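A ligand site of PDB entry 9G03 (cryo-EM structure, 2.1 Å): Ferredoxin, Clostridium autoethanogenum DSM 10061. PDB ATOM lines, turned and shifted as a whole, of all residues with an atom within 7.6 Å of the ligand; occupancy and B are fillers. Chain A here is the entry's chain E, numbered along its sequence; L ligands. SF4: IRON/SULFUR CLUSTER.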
ATOM      1  N   TYR A   3      23.591  -0.473  28.318  1.00  0.00           N
ATOM      2  CA  TYR A   3      25.067  -0.632  28.479  1.00  0.00           C
ATOM      3  C   TYR A   3      25.756   0.725  28.484  1.00  0.00           C
ATOM      4  O   TYR A   3      25.343   1.647  27.782  1.00  0.00           O
ATOM      5  CB  TYR A   3      25.626  -1.499  27.352  1.00  0.00           C
ATOM      6  CG  TYR A   3      26.182  -2.822  27.808  1.00  0.00           C
ATOM      7  CD1 TYR A   3      27.516  -2.936  28.202  1.00  0.00           C
ATOM      8  CD2 TYR A   3      25.398  -3.960  27.850  1.00  0.00           C
ATOM      9  CE1 TYR A   3      28.027  -4.134  28.621  1.00  0.00           C
ATOM     10  CE2 TYR A   3      25.906  -5.166  28.266  1.00  0.00           C
ATOM     11  CZ  TYR A   3      27.223  -5.252  28.645  1.00  0.00           C
ATOM     12  OH  TYR A   3      27.738  -6.453  29.073  1.00  0.00           O
ATOM     13  N   LYS A   4      26.809   0.862  29.287  1.00  0.00           N
ATOM     14  CA  LYS A   4      27.511   2.135  29.409  1.00  0.00           C
ATOM     15  C   LYS A   4      29.016   1.906  29.362  1.00  0.00           C
ATOM     16  O   LYS A   4      29.531   1.005  30.019  1.00  0.00           O
ATOM     17  CB  LYS A   4      27.130   2.856  30.710  1.00  0.00           C
ATOM     18  CG  LYS A   4      25.678   3.304  30.761  1.00  0.00           C
ATOM     19  CD  LYS A   4      25.331   3.980  32.087  1.00  0.00           C
ATOM     20  CE  LYS A   4      23.890   4.465  32.111  1.00  0.00           C
ATOM     21  NZ  LYS A   4      23.520   5.112  33.401  1.00  0.00           N
ATOM     22  N   CYS A  15      34.191  -2.241  19.471  1.00  0.00           N
ATOM     23  CA  CYS A  15      32.787  -2.268  19.858  1.00  0.00           C
ATOM     24  C   CYS A  15      31.950  -1.541  18.831  1.00  0.00           C
ATOM     25  O   CYS A  15      30.842  -1.978  18.506  1.00  0.00           O
ATOM     26  CB  CYS A  15      32.630  -1.638  21.244  1.00  0.00           C
ATOM     27  SG  CYS A  15      33.362   0.007  21.369  1.00  0.00           S
ATOM     28  N   ALA A  16      32.444  -0.413  18.332  1.00  0.00           N
ATOM     29  CA  ALA A  16      31.663   0.400  17.415  1.00  0.00           C
ATOM     30  C   ALA A  16      31.076  -0.490  16.314  1.00  0.00           C
ATOM     31  O   ALA A  16      29.853  -0.628  16.196  1.00  0.00           O
ATOM     32  CB  ALA A  16      32.528   1.513  16.821  1.00  0.00           C
ATOM     33  N   GLU A  18      31.154  -3.776  15.906  1.00  0.00           N
ATOM     34  CA  GLU A  18      30.471  -5.012  16.287  1.00  0.00           C
ATOM     35  C   GLU A  18      29.017  -4.764  16.671  1.00  0.00           C
ATOM     36  O   GLU A  18      28.147  -5.607  16.415  1.00  0.00           O
ATOM     37  CB  GLU A  18      31.223  -5.712  17.404  1.00  0.00           C
ATOM     38  CG  GLU A  18      32.633  -6.121  16.984  1.00  0.00           C
ATOM     39  CD  GLU A  18      32.749  -7.567  16.520  1.00  0.00           C
ATOM     40  OE1 GLU A  18      31.799  -8.348  16.710  1.00  0.00           O
ATOM     41  OE2 GLU A  18      33.809  -7.927  15.958  1.00  0.00           O
ATOM     42  N   CYS A  19      28.739  -3.629  17.296  1.00  0.00           N
ATOM     43  CA  CYS A  19      27.397  -3.224  17.714  1.00  0.00           C
ATOM     44  C   CYS A  19      26.345  -3.527  16.648  1.00  0.00           C
ATOM     45  O   CYS A  19      26.363  -2.918  15.566  1.00  0.00           O
ATOM     46  CB  CYS A  19      27.362  -1.737  18.031  1.00  0.00           C
ATOM     47  SG  CYS A  19      26.002  -1.253  19.107  1.00  0.00           S
ATOM     48  N   PRO A  20      25.424  -4.459  16.910  1.00  0.00           N
ATOM     49  CA  PRO A  20      24.308  -4.684  15.965  1.00  0.00           C
ATOM     50  C   PRO A  20      23.473  -3.450  15.719  1.00  0.00           C
ATOM     51  O   PRO A  20      23.173  -3.121  14.559  1.00  0.00           O
ATOM     52  CB  PRO A  20      23.500  -5.810  16.643  1.00  0.00           C
ATOM     53  CG  PRO A  20      24.419  -6.419  17.634  1.00  0.00           C
ATOM     54  CD  PRO A  20      25.312  -5.318  18.103  1.00  0.00           C
ATOM     55  N   ALA A  21      23.069  -2.745  16.775  1.00  0.00           N
ATOM     56  CA  ALA A  21      22.224  -1.576  16.666  1.00  0.00           C
ATOM     57  C   ALA A  21      23.014  -0.316  16.309  1.00  0.00           C
ATOM     58  O   ALA A  21      22.406   0.731  16.064  1.00  0.00           O
ATOM     59  CB  ALA A  21      21.468  -1.334  17.975  1.00  0.00           C
ATOM     60  N   ASP A  22      24.344  -0.390  16.257  1.00  0.00           N
ATOM     61  CA  ASP A  22      25.188   0.749  15.910  1.00  0.00           C
ATOM     62  C   ASP A  22      24.964   1.927  16.855  1.00  0.00           C
ATOM     63  O   ASP A  22      25.013   3.088  16.436  1.00  0.00           O
ATOM     64  CB  ASP A  22      24.951   1.181  14.457  1.00  0.00           C
ATOM     65  CG  ASP A  22      25.445   0.157  13.461  1.00  0.00           C
ATOM     66  OD1 ASP A  22      26.532  -0.407  13.678  1.00  0.00           O
ATOM     67  OD2 ASP A  22      24.742  -0.089  12.457  1.00  0.00           O
ATOM     68  N   ALA A  23      24.705   1.630  18.119  1.00  0.00           N
ATOM     69  CA  ALA A  23      24.545   2.677  19.114  1.00  0.00           C
ATOM     70  C   ALA A  23      25.867   3.367  19.419  1.00  0.00           C
ATOM     71  O   ALA A  23      25.892   4.551  19.759  1.00  0.00           O
ATOM     72  CB  ALA A  23      23.951   2.100  20.392  1.00  0.00           C
ATOM     73  N   ILE A  24      26.977   2.628  19.309  1.00  0.00           N
ATOM     74  CA  ILE A  24      28.284   3.084  19.762  1.00  0.00           C
ATOM     75  C   ILE A  24      28.892   4.027  18.730  1.00  0.00           C
ATOM     76  O   ILE A  24      28.949   3.708  17.535  1.00  0.00           O
ATOM     77  CB  ILE A  24      29.202   1.891  20.027  1.00  0.00           C
ATOM     78  CG1 ILE A  24      28.493   0.875  20.931  1.00  0.00           C
ATOM     79  CG2 ILE A  24      30.513   2.366  20.651  1.00  0.00           C
ATOM     80  CD1 ILE A  24      29.303  -0.368  21.234  1.00  0.00           C
ATOM     81  N   VAL A  32      31.330   6.245  22.899  1.00  0.00           N
ATOM     82  CA  VAL A  32      30.176   6.409  23.772  1.00  0.00           C
ATOM     83  C   VAL A  32      29.028   5.553  23.265  1.00  0.00           C
ATOM     84  O   VAL A  32      28.953   5.206  22.083  1.00  0.00           O
ATOM     85  CB  VAL A  32      29.753   7.890  23.863  1.00  0.00           C
ATOM     86  CG1 VAL A  32      30.779   8.691  24.652  1.00  0.00           C
ATOM     87  CG2 VAL A  32      29.562   8.486  22.471  1.00  0.00           C
ATOM     88  N   ILE A  33      28.131   5.227  24.190  1.00  0.00           N
ATOM     89  CA  ILE A  33      26.957   4.394  23.944  1.00  0.00           C
ATOM     90  C   ILE A  33      25.671   5.207  24.079  1.00  0.00           C
ATOM     91  O   ILE A  33      25.420   5.805  25.134  1.00  0.00           O
ATOM     92  CB  ILE A  33      26.920   3.199  24.903  1.00  0.00           C
ATOM     93  CG1 ILE A  33      28.102   2.272  24.639  1.00  0.00           C
ATOM     94  CG2 ILE A  33      25.593   2.435  24.764  1.00  0.00           C
ATOM     95  CD1 ILE A  33      28.316   1.245  25.717  1.00  0.00           C
ATOM     96  N   ASP A  34      24.866   5.218  23.022  1.00  0.00           N
ATOM     97  CA  ASP A  34      23.586   5.907  23.060  1.00  0.00           C
ATOM     98  C   ASP A  34      22.600   4.998  23.781  1.00  0.00           C
ATOM     99  O   ASP A  34      22.292   3.909  23.269  1.00  0.00           O
ATOM    100  CB  ASP A  34      23.100   6.240  21.667  1.00  0.00           C
ATOM    101  CG  ASP A  34      21.841   7.110  21.678  1.00  0.00           C
ATOM    102  OD1 ASP A  34      20.841   6.703  22.306  1.00  0.00           O
ATOM    103  OD2 ASP A  34      21.873   8.195  21.074  1.00  0.00           O
ATOM    104  N   PRO A  35      22.075   5.383  24.950  1.00  0.00           N
ATOM    105  CA  PRO A  35      21.162   4.467  25.678  1.00  0.00           C
ATOM    106  C   PRO A  35      19.849   4.195  24.963  1.00  0.00           C
ATOM    107  O   PRO A  35      19.301   3.100  25.134  1.00  0.00           O
ATOM    108  CB  PRO A  35      20.935   5.201  27.008  1.00  0.00           C
ATOM    109  CG  PRO A  35      21.181   6.627  26.702  1.00  0.00           C
ATOM    110  CD  PRO A  35      22.260   6.658  25.668  1.00  0.00           C
ATOM    111  N   LYS A  37      19.130   3.631  21.827  1.00  0.00           N
ATOM    112  CA  LYS A  37      19.202   2.646  20.748  1.00  0.00           C
ATOM    113  C   LYS A  37      20.029   1.407  21.103  1.00  0.00           C
ATOM    114  O   LYS A  37      20.339   0.616  20.219  1.00  0.00           O
ATOM    115  CB  LYS A  37      19.768   3.307  19.491  1.00  0.00           C
ATOM    116  CG  LYS A  37      21.076   4.046  19.703  1.00  0.00           C
ATOM    117  CD  LYS A  37      21.512   4.804  18.467  1.00  0.00           C
ATOM    118  CE  LYS A  37      20.659   6.040  18.232  1.00  0.00           C
ATOM    119  NZ  LYS A  37      21.168   6.877  17.117  1.00  0.00           N
ATOM    120  N   CYS A  38      20.379   1.229  22.375  1.00  0.00           N
ATOM    121  CA  CYS A  38      21.155   0.075  22.812  1.00  0.00           C
ATOM    122  C   CYS A  38      20.202  -1.076  23.129  1.00  0.00           C
ATOM    123  O   CYS A  38      19.317  -0.930  23.972  1.00  0.00           O
ATOM    124  CB  CYS A  38      21.990   0.436  24.039  1.00  0.00           C
ATOM    125  SG  CYS A  38      22.969  -0.903  24.741  1.00  0.00           S
ATOM    126  N   ILE A  39      20.385  -2.220  22.456  1.00  0.00           N
ATOM    127  CA  ILE A  39      19.481  -3.356  22.634  1.00  0.00           C
ATOM    128  C   ILE A  39      19.968  -4.247  23.773  1.00  0.00           C
ATOM    129  O   ILE A  39      19.470  -5.366  23.956  1.00  0.00           O
ATOM    130  CB  ILE A  39      19.349  -4.149  21.305  1.00  0.00           C
ATOM    131  CG1 ILE A  39      18.686  -3.287  20.224  1.00  0.00           C
ATOM    132  CG2 ILE A  39      18.526  -5.429  21.482  1.00  0.00           C
ATOM    133  CD1 ILE A  39      18.714  -3.898  18.830  1.00  0.00           C
ATOM    134  N   GLU A  40      20.893  -3.747  24.587  1.00  0.00           N
ATOM    135  CA  GLU A  40      21.373  -4.475  25.754  1.00  0.00           C
ATOM    136  C   GLU A  40      21.949  -5.850  25.407  1.00  0.00           C
ATOM    137  O   GLU A  40      22.044  -6.723  26.272  1.00  0.00           O
ATOM    138  CB  GLU A  40      20.236  -4.616  26.779  1.00  0.00           C
ATOM    139  CG  GLU A  40      20.588  -5.238  28.136  1.00  0.00           C
ATOM    140  CD  GLU A  40      21.640  -4.456  28.891  1.00  0.00           C
ATOM    141  OE1 GLU A  40      21.857  -3.276  28.546  1.00  0.00           O
ATOM    142  OE2 GLU A  40      22.235  -5.024  29.831  1.00  0.00           O
ATOM    143  N   CYS A  41      22.378  -6.080  24.167  1.00  0.00           N
ATOM    144  CA  CYS A  41      22.916  -7.396  23.826  1.00  0.00           C
ATOM    145  C   CYS A  41      24.186  -7.690  24.604  1.00  0.00           C
ATOM    146  O   CYS A  41      24.397  -8.808  25.092  1.00  0.00           O
ATOM    147  CB  CYS A  41      23.150  -7.518  22.325  1.00  0.00           C
ATOM    148  SG  CYS A  41      24.494  -6.522  21.660  1.00  0.00           S
ATOM    149  N   GLY A  42      25.067  -6.690  24.734  1.00  0.00           N
ATOM    150  CA  GLY A  42      26.325  -6.860  25.410  1.00  0.00           C
ATOM    151  C   GLY A  42      27.451  -7.387  24.537  1.00  0.00           C
ATOM    152  O   GLY A  42      28.516  -7.723  25.076  1.00  0.00           O
ATOM    153  N   ASN A  43      27.244  -7.462  23.227  1.00  0.00           N
ATOM    154  CA  ASN A  43      28.293  -7.913  22.328  1.00  0.00           C
ATOM    155  C   ASN A  43      29.506  -6.988  22.385  1.00  0.00           C
ATOM    156  O   ASN A  43      30.640  -7.444  22.176  1.00  0.00           O
ATOM    157  CB  ASN A  43      27.767  -7.995  20.898  1.00  0.00           C
ATOM    158  CG  ASN A  43      28.713  -8.723  19.975  1.00  0.00           C
ATOM    159  OD1 ASN A  43      29.459  -9.594  20.402  1.00  0.00           O
ATOM    160  ND2 ASN A  43      28.699  -8.354  18.703  1.00  0.00           N
ATOM    161  N   CYS A  44      29.300  -5.709  22.668  1.00  0.00           N
ATOM    162  CA  CYS A  44      30.422  -4.779  22.787  1.00  0.00           C
ATOM    163  C   CYS A  44      31.327  -5.166  23.951  1.00  0.00           C
ATOM    164  O   CYS A  44      32.559  -5.155  23.815  1.00  0.00           O
ATOM    165  CB  CYS A  44      29.891  -3.359  22.961  1.00  0.00           C
ATOM    166  SG  CYS A  44      28.671  -3.197  24.272  1.00  0.00           S
ATOM    167  N   ALA A  45      30.740  -5.507  25.086  1.00  0.00           N
ATOM    168  CA  ALA A  45      31.535  -5.958  26.225  1.00  0.00           C
ATOM    169  C   ALA A  45      32.385  -7.160  25.833  1.00  0.00           C
ATOM    170  O   ALA A  45      33.560  -7.267  26.207  1.00  0.00           O
ATOM    171  CB  ALA A  45      30.641  -6.298  27.405  1.00  0.00           C
ATOM    172  N   ASN A  46      31.798  -8.082  25.065  1.00  0.00           N
ATOM    173  CA  ASN A  46      32.516  -9.262  24.619  1.00  0.00           C
ATOM    174  C   ASN A  46      33.703  -8.893  23.735  1.00  0.00           C
ATOM    175  O   ASN A  46      34.784  -9.464  23.858  1.00  0.00           O
ATOM    176  CB  ASN A  46      31.547 -10.184  23.887  1.00  0.00           C
ATOM    177  CG  ASN A  46      32.119 -11.562  23.636  1.00  0.00           C
ATOM    178  OD1 ASN A  46      32.952 -12.051  24.395  1.00  0.00           O
ATOM    179  ND2 ASN A  46      31.677 -12.192  22.554  1.00  0.00           N
ATOM    180  N   VAL A  47      33.520  -7.908  22.839  1.00  0.00           N
ATOM    181  CA  VAL A  47      34.536  -7.524  21.873  1.00  0.00           C
ATOM    182  C   VAL A  47      35.284  -6.305  22.415  1.00  0.00           C
ATOM    183  O   VAL A  47      35.185  -5.205  21.862  1.00  0.00           O
ATOM    184  CB  VAL A  47      33.948  -7.223  20.486  1.00  0.00           C
ATOM    185  CG1 VAL A  47      35.081  -7.176  19.465  1.00  0.00           C
ATOM    186  CG2 VAL A  47      32.914  -8.246  20.084  1.00  0.00           C
ATOM    187  N   PRO A  53      33.317  -1.587  28.121  1.00  0.00           N
ATOM    188  CA  PRO A  53      31.849  -1.504  28.131  1.00  0.00           C
ATOM    189  C   PRO A  53      31.247  -2.254  29.314  1.00  0.00           C
ATOM    190  O   PRO A  53      31.418  -3.466  29.455  1.00  0.00           O
ATOM    191  CB  PRO A  53      31.452  -2.155  26.803  1.00  0.00           C
ATOM    192  CG  PRO A  53      32.678  -2.179  25.980  1.00  0.00           C
ATOM    193  CD  PRO A  53      33.810  -2.310  26.940  1.00  0.00           C
HETATM  194 FE1  SF4 L   1      24.069  -2.030  23.304  1.00  0.00          FE
HETATM  195 FE2  SF4 L   1      24.658  -4.463  22.214  1.00  0.00          FE
HETATM  196 FE3  SF4 L   1      26.635  -2.974  23.384  1.00  0.00          FE
HETATM  197 FE4  SF4 L   1      25.545  -2.175  21.007  1.00  0.00          FE
HETATM  198  S1  SF4 L   1      26.748  -4.071  21.385  1.00  0.00           S
HETATM  199  S2  SF4 L   1      25.979  -0.867  22.830  1.00  0.00           S
HETATM  200  S3  SF4 L   1      23.379  -2.821  21.283  1.00  0.00           S
HETATM  201  S4  SF4 L   1      24.808  -3.883  24.407  1.00  0.00           S
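The side-chain sulfur of Cys 41 binds an iron atom (FE2) of the ligand. The side-chain sulfur of Cys 38 is bound to an iron atom (FE1) of the ligand, at 2.1 Å. The backbone NH of Gly 42 lies close to a sulfur (S4) of the ligand (2.8 Å). SG of Cys 19 binds FE4 of the ligand. S1 of the ligand lies close to N of Cys 44 (3.3 Å). The backbone NH of Ile 39 sits close to a sulfur (S3) of the ligand (3.3 Å). FE3 of the ligand is bound by SG of Cys 44, at 2.2 Å. S4 of the ligand sits close to N of Cys 41, at 3.3 Å.
The side-chain sulfur (SG) of Cys 38 lies close to the backbone NH (N) of Glu 40 (3.5 Å). The side-chain carboxylate of Glu 40 lies within hydrogen-bond range of the backbone NH of Tyr 3 (3.3 Å). The side-chain sulfur (SG) of Cys 19 sits close to the backbone NH (N) of Asp 22, at 3.4 Å. SG of Cys 38 lies close to N of Tyr 3, at 3.7 Å. The side-chain sulfur of Cys 41 lies close to the backbone NH of Asn 43 (3.3 Å). The side-chain sulfur (SG) of Cys 19 lies close to the backbone NH (N) of Ala 23, at 3.3 Å.
Merely in contact with the ligand: Tyr 3 (3.5 Å), Pro 20 (3.8 Å), Ile 24 (3.6 Å), Ile 33 (3.8 Å), Glu 40 (3.6 Å) and Asn 43 (3.9 Å). Hydrophobic or aromatic side chains within 4 Å of the ligand: Tyr 3, Pro 20, Ile 24 and Ile 33. Within 4 Å of the ligand: Tyr 3, Cys 19, Pro 20, Ile 24, Ile 33, Cys 38, Ile 39, Glu 40, Cys 41, Gly 42, Asn 43 and Cys 44.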
